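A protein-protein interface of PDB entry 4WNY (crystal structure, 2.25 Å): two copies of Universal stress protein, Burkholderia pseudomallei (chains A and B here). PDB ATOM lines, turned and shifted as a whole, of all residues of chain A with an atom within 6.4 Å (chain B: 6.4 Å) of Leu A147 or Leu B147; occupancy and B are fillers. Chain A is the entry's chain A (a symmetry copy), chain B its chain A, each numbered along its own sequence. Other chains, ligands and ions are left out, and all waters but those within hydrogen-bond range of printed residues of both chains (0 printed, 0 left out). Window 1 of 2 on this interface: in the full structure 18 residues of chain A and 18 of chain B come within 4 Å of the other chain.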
ATOM      1  N   TYR A   6     -35.110 -31.890   8.692  1.00  0.00           N
ATOM      2  CA  TYR A   6     -34.788 -30.794   7.796  1.00  0.00           C
ATOM      3  C   TYR A   6     -35.975 -30.460   6.905  1.00  0.00           C
ATOM      4  O   TYR A   6     -35.795 -29.999   5.785  1.00  0.00           O
ATOM      5  CB  TYR A   6     -33.569 -31.140   6.941  1.00  0.00           C
ATOM      6  CG  TYR A   6     -32.339 -31.496   7.744  1.00  0.00           C
ATOM      7  CD1 TYR A   6     -31.613 -30.516   8.406  1.00  0.00           C
ATOM      8  CD2 TYR A   6     -31.902 -32.811   7.834  1.00  0.00           C
ATOM      9  CE1 TYR A   6     -30.487 -30.835   9.141  1.00  0.00           C
ATOM     10  CE2 TYR A   6     -30.776 -33.140   8.567  1.00  0.00           C
ATOM     11  CZ  TYR A   6     -30.072 -32.148   9.217  1.00  0.00           C
ATOM     12  OH  TYR A   6     -28.950 -32.465   9.948  1.00  0.00           O
ATOM     13  N   ALA A  25     -27.625 -21.180  -1.309  1.00  0.00           N
ATOM     14  CA  ALA A  25     -27.194 -22.399  -0.636  1.00  0.00           C
ATOM     15  C   ALA A  25     -28.370 -23.080   0.053  1.00  0.00           C
ATOM     16  O   ALA A  25     -28.513 -24.302  -0.006  1.00  0.00           O
ATOM     17  CB  ALA A  25     -26.095 -22.089   0.366  1.00  0.00           C
ATOM     18  N   ALA A  26     -29.209 -22.279   0.706  1.00  0.00           N
ATOM     19  CA  ALA A  26     -30.395 -22.788   1.384  1.00  0.00           C
ATOM     20  C   ALA A  26     -31.384 -23.369   0.378  1.00  0.00           C
ATOM     21  O   ALA A  26     -32.036 -24.376   0.648  1.00  0.00           O
ATOM     22  CB  ALA A  26     -31.053 -21.690   2.206  1.00  0.00           C
ATOM     23  N   LEU A  29     -30.067 -26.727  -0.867  1.00  0.00           N
ATOM     24  CA  LEU A  29     -30.298 -27.715   0.177  1.00  0.00           C
ATOM     25  C   LEU A  29     -31.770 -28.100   0.239  1.00  0.00           C
ATOM     26  O   LEU A  29     -32.108 -29.273   0.387  1.00  0.00           O
ATOM     27  CB  LEU A  29     -29.838 -27.182   1.534  1.00  0.00           C
ATOM     28  CG  LEU A  29     -29.928 -28.167   2.696  1.00  0.00           C
ATOM     29  CD1 LEU A  29     -28.867 -29.240   2.551  1.00  0.00           C
ATOM     30  CD2 LEU A  29     -29.791 -27.448   4.024  1.00  0.00           C
ATOM     31  N   LEU A 115     -34.029 -25.750  11.161  1.00  0.00           N
ATOM     32  CA  LEU A 115     -32.715 -25.305  10.714  1.00  0.00           C
ATOM     33  C   LEU A 115     -32.721 -23.824  10.351  1.00  0.00           C
ATOM     34  O   LEU A 115     -33.653 -23.339   9.709  1.00  0.00           O
ATOM     35  CB  LEU A 115     -32.248 -26.128   9.512  1.00  0.00           C
ATOM     36  CG  LEU A 115     -30.925 -25.695   8.873  1.00  0.00           C
ATOM     37  CD1 LEU A 115     -29.772 -25.867   9.854  1.00  0.00           C
ATOM     38  CD2 LEU A 115     -30.670 -26.467   7.586  1.00  0.00           C
ATOM     39  N   ILE A 116     -31.676 -23.114  10.763  1.00  0.00           N
ATOM     40  CA  ILE A 116     -31.510 -21.711  10.404  1.00  0.00           C
ATOM     41  C   ILE A 116     -30.252 -21.517   9.566  1.00  0.00           C
ATOM     42  O   ILE A 116     -29.153 -21.891   9.980  1.00  0.00           O
ATOM     43  CB  ILE A 116     -31.426 -20.810  11.650  1.00  0.00           C
ATOM     44  CG1 ILE A 116     -32.745 -20.841  12.423  1.00  0.00           C
ATOM     45  CG2 ILE A 116     -31.077 -19.381  11.253  1.00  0.00           C
ATOM     46  CD1 ILE A 116     -32.735 -19.984  13.669  1.00  0.00           C
ATOM     47  N   VAL A 117     -30.419 -20.931   8.386  1.00  0.00           N
ATOM     48  CA  VAL A 117     -29.304 -20.705   7.478  1.00  0.00           C
ATOM     49  C   VAL A 117     -28.911 -19.231   7.469  1.00  0.00           C
ATOM     50  O   VAL A 117     -29.765 -18.358   7.320  1.00  0.00           O
ATOM     51  CB  VAL A 117     -29.657 -21.163   6.048  1.00  0.00           C
ATOM     52  CG1 VAL A 117     -28.569 -20.752   5.065  1.00  0.00           C
ATOM     53  CG2 VAL A 117     -29.876 -22.670   6.020  1.00  0.00           C
ATOM     54  N   MET A 118     -27.621 -18.958   7.639  1.00  0.00           N
ATOM     55  CA  MET A 118     -27.127 -17.587   7.689  1.00  0.00           C
ATOM     56  C   MET A 118     -25.896 -17.375   6.823  1.00  0.00           C
ATOM     57  O   MET A 118     -25.065 -18.272   6.677  1.00  0.00           O
ATOM     58  CB  MET A 118     -26.792 -17.192   9.127  1.00  0.00           C
ATOM     59  CG  MET A 118     -27.825 -16.302   9.787  1.00  0.00           C
ATOM     60  SD  MET A 118     -27.260 -15.803  11.418  1.00  0.00           S
ATOM     61  CE  MET A 118     -26.660 -17.379  12.016  1.00  0.00           C
ATOM     62  N   GLY A 119     -25.779 -16.179   6.258  1.00  0.00           N
ATOM     63  CA  GLY A 119     -24.584 -15.794   5.533  1.00  0.00           C
ATOM     64  C   GLY A 119     -23.607 -15.119   6.474  1.00  0.00           C
ATOM     65  O   GLY A 119     -24.005 -14.304   7.307  1.00  0.00           O
ATOM     66  N   PRO A 145     -30.332 -25.775  15.420  1.00  0.00           N
ATOM     67  CA  PRO A 145     -29.290 -26.011  14.410  1.00  0.00           C
ATOM     68  C   PRO A 145     -29.063 -24.811  13.493  1.00  0.00           C
ATOM     69  O   PRO A 145     -30.025 -24.247  12.974  1.00  0.00           O
ATOM     70  CB  PRO A 145     -29.841 -27.199  13.617  1.00  0.00           C
ATOM     71  CG  PRO A 145     -30.693 -27.924  14.584  1.00  0.00           C
ATOM     72  CD  PRO A 145     -31.329 -26.861  15.438  1.00  0.00           C
ATOM     73  N   VAL A 146     -27.803 -24.426  13.302  1.00  0.00           N
ATOM     74  CA  VAL A 146     -27.465 -23.265  12.482  1.00  0.00           C
ATOM     75  C   VAL A 146     -26.436 -23.615  11.406  1.00  0.00           C
ATOM     76  O   VAL A 146     -25.425 -24.261  11.686  1.00  0.00           O
ATOM     77  CB  VAL A 146     -26.910 -22.108  13.345  1.00  0.00           C
ATOM     78  CG1 VAL A 146     -26.583 -20.913  12.476  1.00  0.00           C
ATOM     79  CG2 VAL A 146     -27.900 -21.719  14.434  1.00  0.00           C
ATOM     80  N   LEU A 147     -26.698 -23.182  10.176  1.00  0.00           N
ATOM     81  CA  LEU A 147     -25.795 -23.426   9.060  1.00  0.00           C
ATOM     82  C   LEU A 147     -25.155 -22.130   8.580  1.00  0.00           C
ATOM     83  O   LEU A 147     -25.843 -21.234   8.089  1.00  0.00           O
ATOM     84  CB  LEU A 147     -26.542 -24.101   7.907  1.00  0.00           C
ATOM     85  CG  LEU A 147     -25.744 -24.385   6.632  1.00  0.00           C
ATOM     86  CD1 LEU A 147     -24.502 -25.207   6.942  1.00  0.00           C
ATOM     87  CD2 LEU A 147     -26.608 -25.076   5.583  1.00  0.00           C
ATOM     88  N   MET A 148     -23.837 -22.038   8.718  1.00  0.00           N
ATOM     89  CA  MET A 148     -23.105 -20.840   8.321  1.00  0.00           C
ATOM     90  C   MET A 148     -22.547 -20.954   6.906  1.00  0.00           C
ATOM     91  O   MET A 148     -21.784 -21.873   6.611  1.00  0.00           O
ATOM     92  CB  MET A 148     -21.955 -20.571   9.292  1.00  0.00           C
ATOM     93  CG  MET A 148     -22.254 -20.896  10.748  1.00  0.00           C
ATOM     94  SD  MET A 148     -23.268 -19.673  11.600  1.00  0.00           S
ATOM     95  CE  MET A 148     -23.088 -20.224  13.297  1.00  0.00           C
ATOM     96  N   ILE A 149     -22.914 -20.020   6.035  1.00  0.00           N
ATOM     97  CA  ILE A 149     -22.323 -19.967   4.702  1.00  0.00           C
ATOM     98  C   ILE A 149     -21.492 -18.699   4.561  1.00  0.00           C
ATOM     99  O   ILE A 149     -22.030 -17.589   4.573  1.00  0.00           O
ATOM    100  CB  ILE A 149     -23.388 -20.020   3.579  1.00  0.00           C
ATOM    101  CG1 ILE A 149     -23.986 -21.428   3.471  1.00  0.00           C
ATOM    102  CG2 ILE A 149     -22.777 -19.598   2.243  1.00  0.00           C
ATOM    103  CD1 ILE A 149     -25.081 -21.712   4.465  1.00  0.00           C
ATOM    104  N   TYR B   6     -23.532 -30.108  -1.749  1.00  0.00           N
ATOM    105  CA  TYR B   6     -23.618 -30.908  -0.541  1.00  0.00           C
ATOM    106  C   TYR B   6     -23.333 -32.371  -0.843  1.00  0.00           C
ATOM    107  O   TYR B   6     -23.848 -33.253  -0.168  1.00  0.00           O
ATOM    108  CB  TYR B   6     -24.996 -30.762   0.103  1.00  0.00           C
ATOM    109  CG  TYR B   6     -25.371 -29.335   0.431  1.00  0.00           C
ATOM    110  CD1 TYR B   6     -24.786 -28.674   1.503  1.00  0.00           C
ATOM    111  CD2 TYR B   6     -26.313 -28.652  -0.327  1.00  0.00           C
ATOM    112  CE1 TYR B   6     -25.125 -27.371   1.809  1.00  0.00           C
ATOM    113  CE2 TYR B   6     -26.659 -27.346  -0.028  1.00  0.00           C
ATOM    114  CZ  TYR B   6     -26.063 -26.712   1.042  1.00  0.00           C
ATOM    115  OH  TYR B   6     -26.401 -25.413   1.348  1.00  0.00           O
ATOM    116  N   ALA B  25     -27.467 -36.374  12.948  1.00  0.00           N
ATOM    117  CA  ALA B  25     -27.992 -35.274  12.151  1.00  0.00           C
ATOM    118  C   ALA B  25     -27.333 -35.240  10.776  1.00  0.00           C
ATOM    119  O   ALA B  25     -28.002 -35.034   9.762  1.00  0.00           O
ATOM    120  CB  ALA B  25     -27.788 -33.952  12.872  1.00  0.00           C
ATOM    121  N   ALA B  26     -26.019 -35.445  10.753  1.00  0.00           N
ATOM    122  CA  ALA B  26     -25.262 -35.473   9.507  1.00  0.00           C
ATOM    123  C   ALA B  26     -25.685 -36.659   8.646  1.00  0.00           C
ATOM    124  O   ALA B  26     -25.753 -36.554   7.422  1.00  0.00           O
ATOM    125  CB  ALA B  26     -23.768 -35.525   9.791  1.00  0.00           C
ATOM    126  N   LEU B  29     -29.102 -35.931   7.112  1.00  0.00           N
ATOM    127  CA  LEU B  29     -28.911 -34.992   6.015  1.00  0.00           C
ATOM    128  C   LEU B  29     -28.307 -35.694   4.807  1.00  0.00           C
ATOM    129  O   LEU B  29     -28.715 -35.455   3.671  1.00  0.00           O
ATOM    130  CB  LEU B  29     -28.017 -33.832   6.449  1.00  0.00           C
ATOM    131  CG  LEU B  29     -27.828 -32.722   5.418  1.00  0.00           C
ATOM    132  CD1 LEU B  29     -29.108 -31.924   5.273  1.00  0.00           C
ATOM    133  CD2 LEU B  29     -26.670 -31.820   5.803  1.00  0.00           C
ATOM    134  N   LEU B 115     -19.037 -29.268   3.156  1.00  0.00           N
ATOM    135  CA  LEU B 115     -19.758 -28.971   4.389  1.00  0.00           C
ATOM    136  C   LEU B 115     -19.119 -29.660   5.589  1.00  0.00           C
ATOM    137  O   LEU B 115     -18.731 -30.825   5.511  1.00  0.00           O
ATOM    138  CB  LEU B 115     -21.223 -29.397   4.270  1.00  0.00           C
ATOM    139  CG  LEU B 115     -22.073 -29.239   5.534  1.00  0.00           C
ATOM    140  CD1 LEU B 115     -22.191 -27.770   5.924  1.00  0.00           C
ATOM    141  CD2 LEU B 115     -23.447 -29.867   5.342  1.00  0.00           C
ATOM    142  N   ILE B 116     -19.014 -28.932   6.697  1.00  0.00           N
ATOM    143  CA  ILE B 116     -18.510 -29.495   7.943  1.00  0.00           C
ATOM    144  C   ILE B 116     -19.587 -29.462   9.021  1.00  0.00           C
ATOM    145  O   ILE B 116     -20.139 -28.405   9.329  1.00  0.00           O
ATOM    146  CB  ILE B 116     -17.269 -28.738   8.449  1.00  0.00           C
ATOM    147  CG1 ILE B 116     -16.106 -28.902   7.471  1.00  0.00           C
ATOM    148  CG2 ILE B 116     -16.871 -29.232   9.835  1.00  0.00           C
ATOM    149  CD1 ILE B 116     -14.851 -28.174   7.899  1.00  0.00           C
ATOM    150  N   VAL B 117     -19.880 -30.624   9.592  1.00  0.00           N
ATOM    151  CA  VAL B 117     -20.904 -30.737  10.620  1.00  0.00           C
ATOM    152  C   VAL B 117     -20.265 -30.920  11.994  1.00  0.00           C
ATOM    153  O   VAL B 117     -19.392 -31.769  12.168  1.00  0.00           O
ATOM    154  CB  VAL B 117     -21.857 -31.912  10.323  1.00  0.00           C
ATOM    155  CG1 VAL B 117     -22.804 -32.149  11.492  1.00  0.00           C
ATOM    156  CG2 VAL B 117     -22.631 -31.648   9.038  1.00  0.00           C
ATOM    157  N   MET B 118     -20.694 -30.116  12.961  1.00  0.00           N
ATOM    158  CA  MET B 118     -20.134 -30.166  14.307  1.00  0.00           C
ATOM    159  C   MET B 118     -21.204 -30.175  15.388  1.00  0.00           C
ATOM    160  O   MET B 118     -22.259 -29.559  15.237  1.00  0.00           O
ATOM    161  CB  MET B 118     -19.204 -28.978  14.543  1.00  0.00           C
ATOM    162  CG  MET B 118     -17.729 -29.313  14.467  1.00  0.00           C
ATOM    163  SD  MET B 118     -16.743 -27.872  14.888  1.00  0.00           S
ATOM    164  CE  MET B 118     -17.613 -26.634  13.934  1.00  0.00           C
ATOM    165  N   GLY B 119     -20.918 -30.869  16.484  1.00  0.00           N
ATOM    166  CA  GLY B 119     -21.781 -30.837  17.649  1.00  0.00           C
ATOM    167  C   GLY B 119     -21.337 -29.734  18.587  1.00  0.00           C
ATOM    168  O   GLY B 119     -20.140 -29.548  18.811  1.00  0.00           O
ATOM    169  N   PRO B 145     -18.426 -23.851   4.597  1.00  0.00           N
ATOM    170  CA  PRO B 145     -19.740 -23.956   5.246  1.00  0.00           C
ATOM    171  C   PRO B 145     -19.728 -24.857   6.480  1.00  0.00           C
ATOM    172  O   PRO B 145     -19.203 -25.968   6.421  1.00  0.00           O
ATOM    173  CB  PRO B 145     -20.620 -24.559   4.147  1.00  0.00           C
ATOM    174  CG  PRO B 145     -19.990 -24.113   2.886  1.00  0.00           C
ATOM    175  CD  PRO B 145     -18.509 -24.117   3.150  1.00  0.00           C
ATOM    176  N   VAL B 146     -20.298 -24.378   7.583  1.00  0.00           N
ATOM    177  CA  VAL B 146     -20.309 -25.129   8.836  1.00  0.00           C
ATOM    178  C   VAL B 146     -21.724 -25.262   9.402  1.00  0.00           C
ATOM    179  O   VAL B 146     -22.469 -24.284   9.473  1.00  0.00           O
ATOM    180  CB  VAL B 146     -19.407 -24.463   9.900  1.00  0.00           C
ATOM    181  CG1 VAL B 146     -19.422 -25.267  11.183  1.00  0.00           C
ATOM    182  CG2 VAL B 146     -17.982 -24.309   9.387  1.00  0.00           C
ATOM    183  N   LEU B 147     -22.086 -26.476   9.806  1.00  0.00           N
ATOM    184  CA  LEU B 147     -23.396 -26.742  10.384  1.00  0.00           C
ATOM    185  C   LEU B 147     -23.281 -27.094  11.862  1.00  0.00           C
ATOM    186  O   LEU B 147     -22.694 -28.115  12.220  1.00  0.00           O
ATOM    187  CB  LEU B 147     -24.093 -27.875   9.626  1.00  0.00           C
ATOM    188  CG  LEU B 147     -25.467 -28.312  10.139  1.00  0.00           C
ATOM    189  CD1 LEU B 147     -26.421 -27.129  10.211  1.00  0.00           C
ATOM    190  CD2 LEU B 147     -26.047 -29.429   9.279  1.00  0.00           C
ATOM    191  N   MET B 148     -23.851 -26.249  12.714  1.00  0.00           N
ATOM    192  CA  MET B 148     -23.792 -26.458  14.156  1.00  0.00           C
ATOM    193  C   MET B 148     -25.025 -27.188  14.679  1.00  0.00           C
ATOM    194  O   MET B 148     -26.148 -26.720  14.498  1.00  0.00           O
ATOM    195  CB  MET B 148     -23.658 -25.120  14.883  1.00  0.00           C
ATOM    196  CG  MET B 148     -22.794 -24.086  14.175  1.00  0.00           C
ATOM    197  SD  MET B 148     -21.019 -24.357  14.331  1.00  0.00           S
ATOM    198  CE  MET B 148     -20.395 -22.799  13.698  1.00  0.00           C
ATOM    199  N   ILE B 149     -24.820 -28.325  15.336  1.00  0.00           N
ATOM    200  CA  ILE B 149     -25.923 -29.020  15.990  1.00  0.00           C
ATOM    201  C   ILE B 149     -25.720 -28.994  17.500  1.00  0.00           C
ATOM    202  O   ILE B 149     -24.781 -29.600  18.019  1.00  0.00           O
ATOM    203  CB  ILE B 149     -26.071 -30.484  15.509  1.00  0.00           C
ATOM    204  CG1 ILE B 149     -26.633 -30.527  14.084  1.00  0.00           C
ATOM    205  CG2 ILE B 149     -26.974 -31.271  16.461  1.00  0.00           C
ATOM    206  CD1 ILE B 149     -25.601 -30.322  13.007  1.00  0.00           C
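The backbone carbonyl oxygen (O) of Val A146 sits at hydrogen-bond distance from the backbone NH (N) of Met B148 (2.7 Å). The backbone NH (N) of Met A148 sits at hydrogen-bond distance from the backbone carbonyl oxygen (O) of Val B146, 2.7 Å away. O of Ala A25 lies within hydrogen-bond range of OH of Tyr B6, 2.7 Å away. The side-chain hydroxyl (OH) of Tyr A6 sits at hydrogen-bond distance from the backbone carbonyl oxygen (O) of Ala B25, 2.7 Å away.
O of Pro A145 lies within hydrogen-bond range of N of Ile A116 (3.0 Å). O of Ile B116 lies within hydrogen-bond range of N of Leu B147, 2.8 Å away. The backbone carbonyl oxygen of Pro B145 is in hydrogen-bond range of the backbone NH of Ile B116 (3.0 Å). N of Met B118 sits at hydrogen-bond distance from O of Leu B147 (2.9 Å). N of Met A118 sits at hydrogen-bond distance from O of Leu A147. The backbone NH (N) of Leu A147 sits at hydrogen-bond distance from the backbone carbonyl oxygen (O) of Ile A116 (2.8 Å).
Among the printed residues, merely in contact across the chains: Tyr A6 with Leu B29 (3.5 Å), Leu A29 with Tyr B6 (3.5 Å), Leu A29 with Leu B29 (3.8 Å), Leu A115 with Leu B147 (3.6 Å), Pro A145 with Met B148 (3.2 Å), Val A146 with Val B146 (3.7 Å), Val A146 with Leu B147 (3.4 Å), Leu A147 with Leu B115 (3.6 Å), Leu A147 with Val B146 (3.4 Å), Leu A147 with Leu B147 (3.8 Å), Met A148 with Pro B145 (3.2 Å) and Met A148 with Met B148 (3.7 Å).
Printed residues of chain B within 4 Å of Ala A25: Tyr B6. Printed residues of chain B within 4 Å of Leu A115: Leu B147. Gly A119 touches none of the printed residues of chain B. Leu A147 touches just these residues of chain B: Leu B115 (3.6 Å), Val B146 (3.4 Å) and Leu B147 (3.8 Å). Printed residues of chain A within 4 Å of Leu B29: Tyr A6 and Leu A29. Leu B147 touches just these residues of chain A: Leu A115 (3.6 Å), Val A146 (3.4 Å) and Leu A147 (3.8 Å). The nearest residue of chain B that does not touch Leu A147 is Tyr B6 (4.3 Å).
Of the 14 printed residues of chain A, 8 touch a printed residue of chain B. Printed residues of chain A that touch a printed residue of chain B: Tyr A6, Ala A25, Leu A29, Leu A115, Pro A145, Val A146, Leu A147 and Met A148. Among the printed residues, 16 pairs touch across the chains.
Tyr A6 touches Leu B29, and with the chains exchanged Leu A29 touches Tyr B6. Leu B29 touches its own counterpart, Leu A29. Leu B147 touches its own counterpart, Leu A147. Met B148 touches its own counterpart, Met A148. Of the 16 pairs that touch across the chains among the printed residues, 16 have their exchanged pair printed and touching as well.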
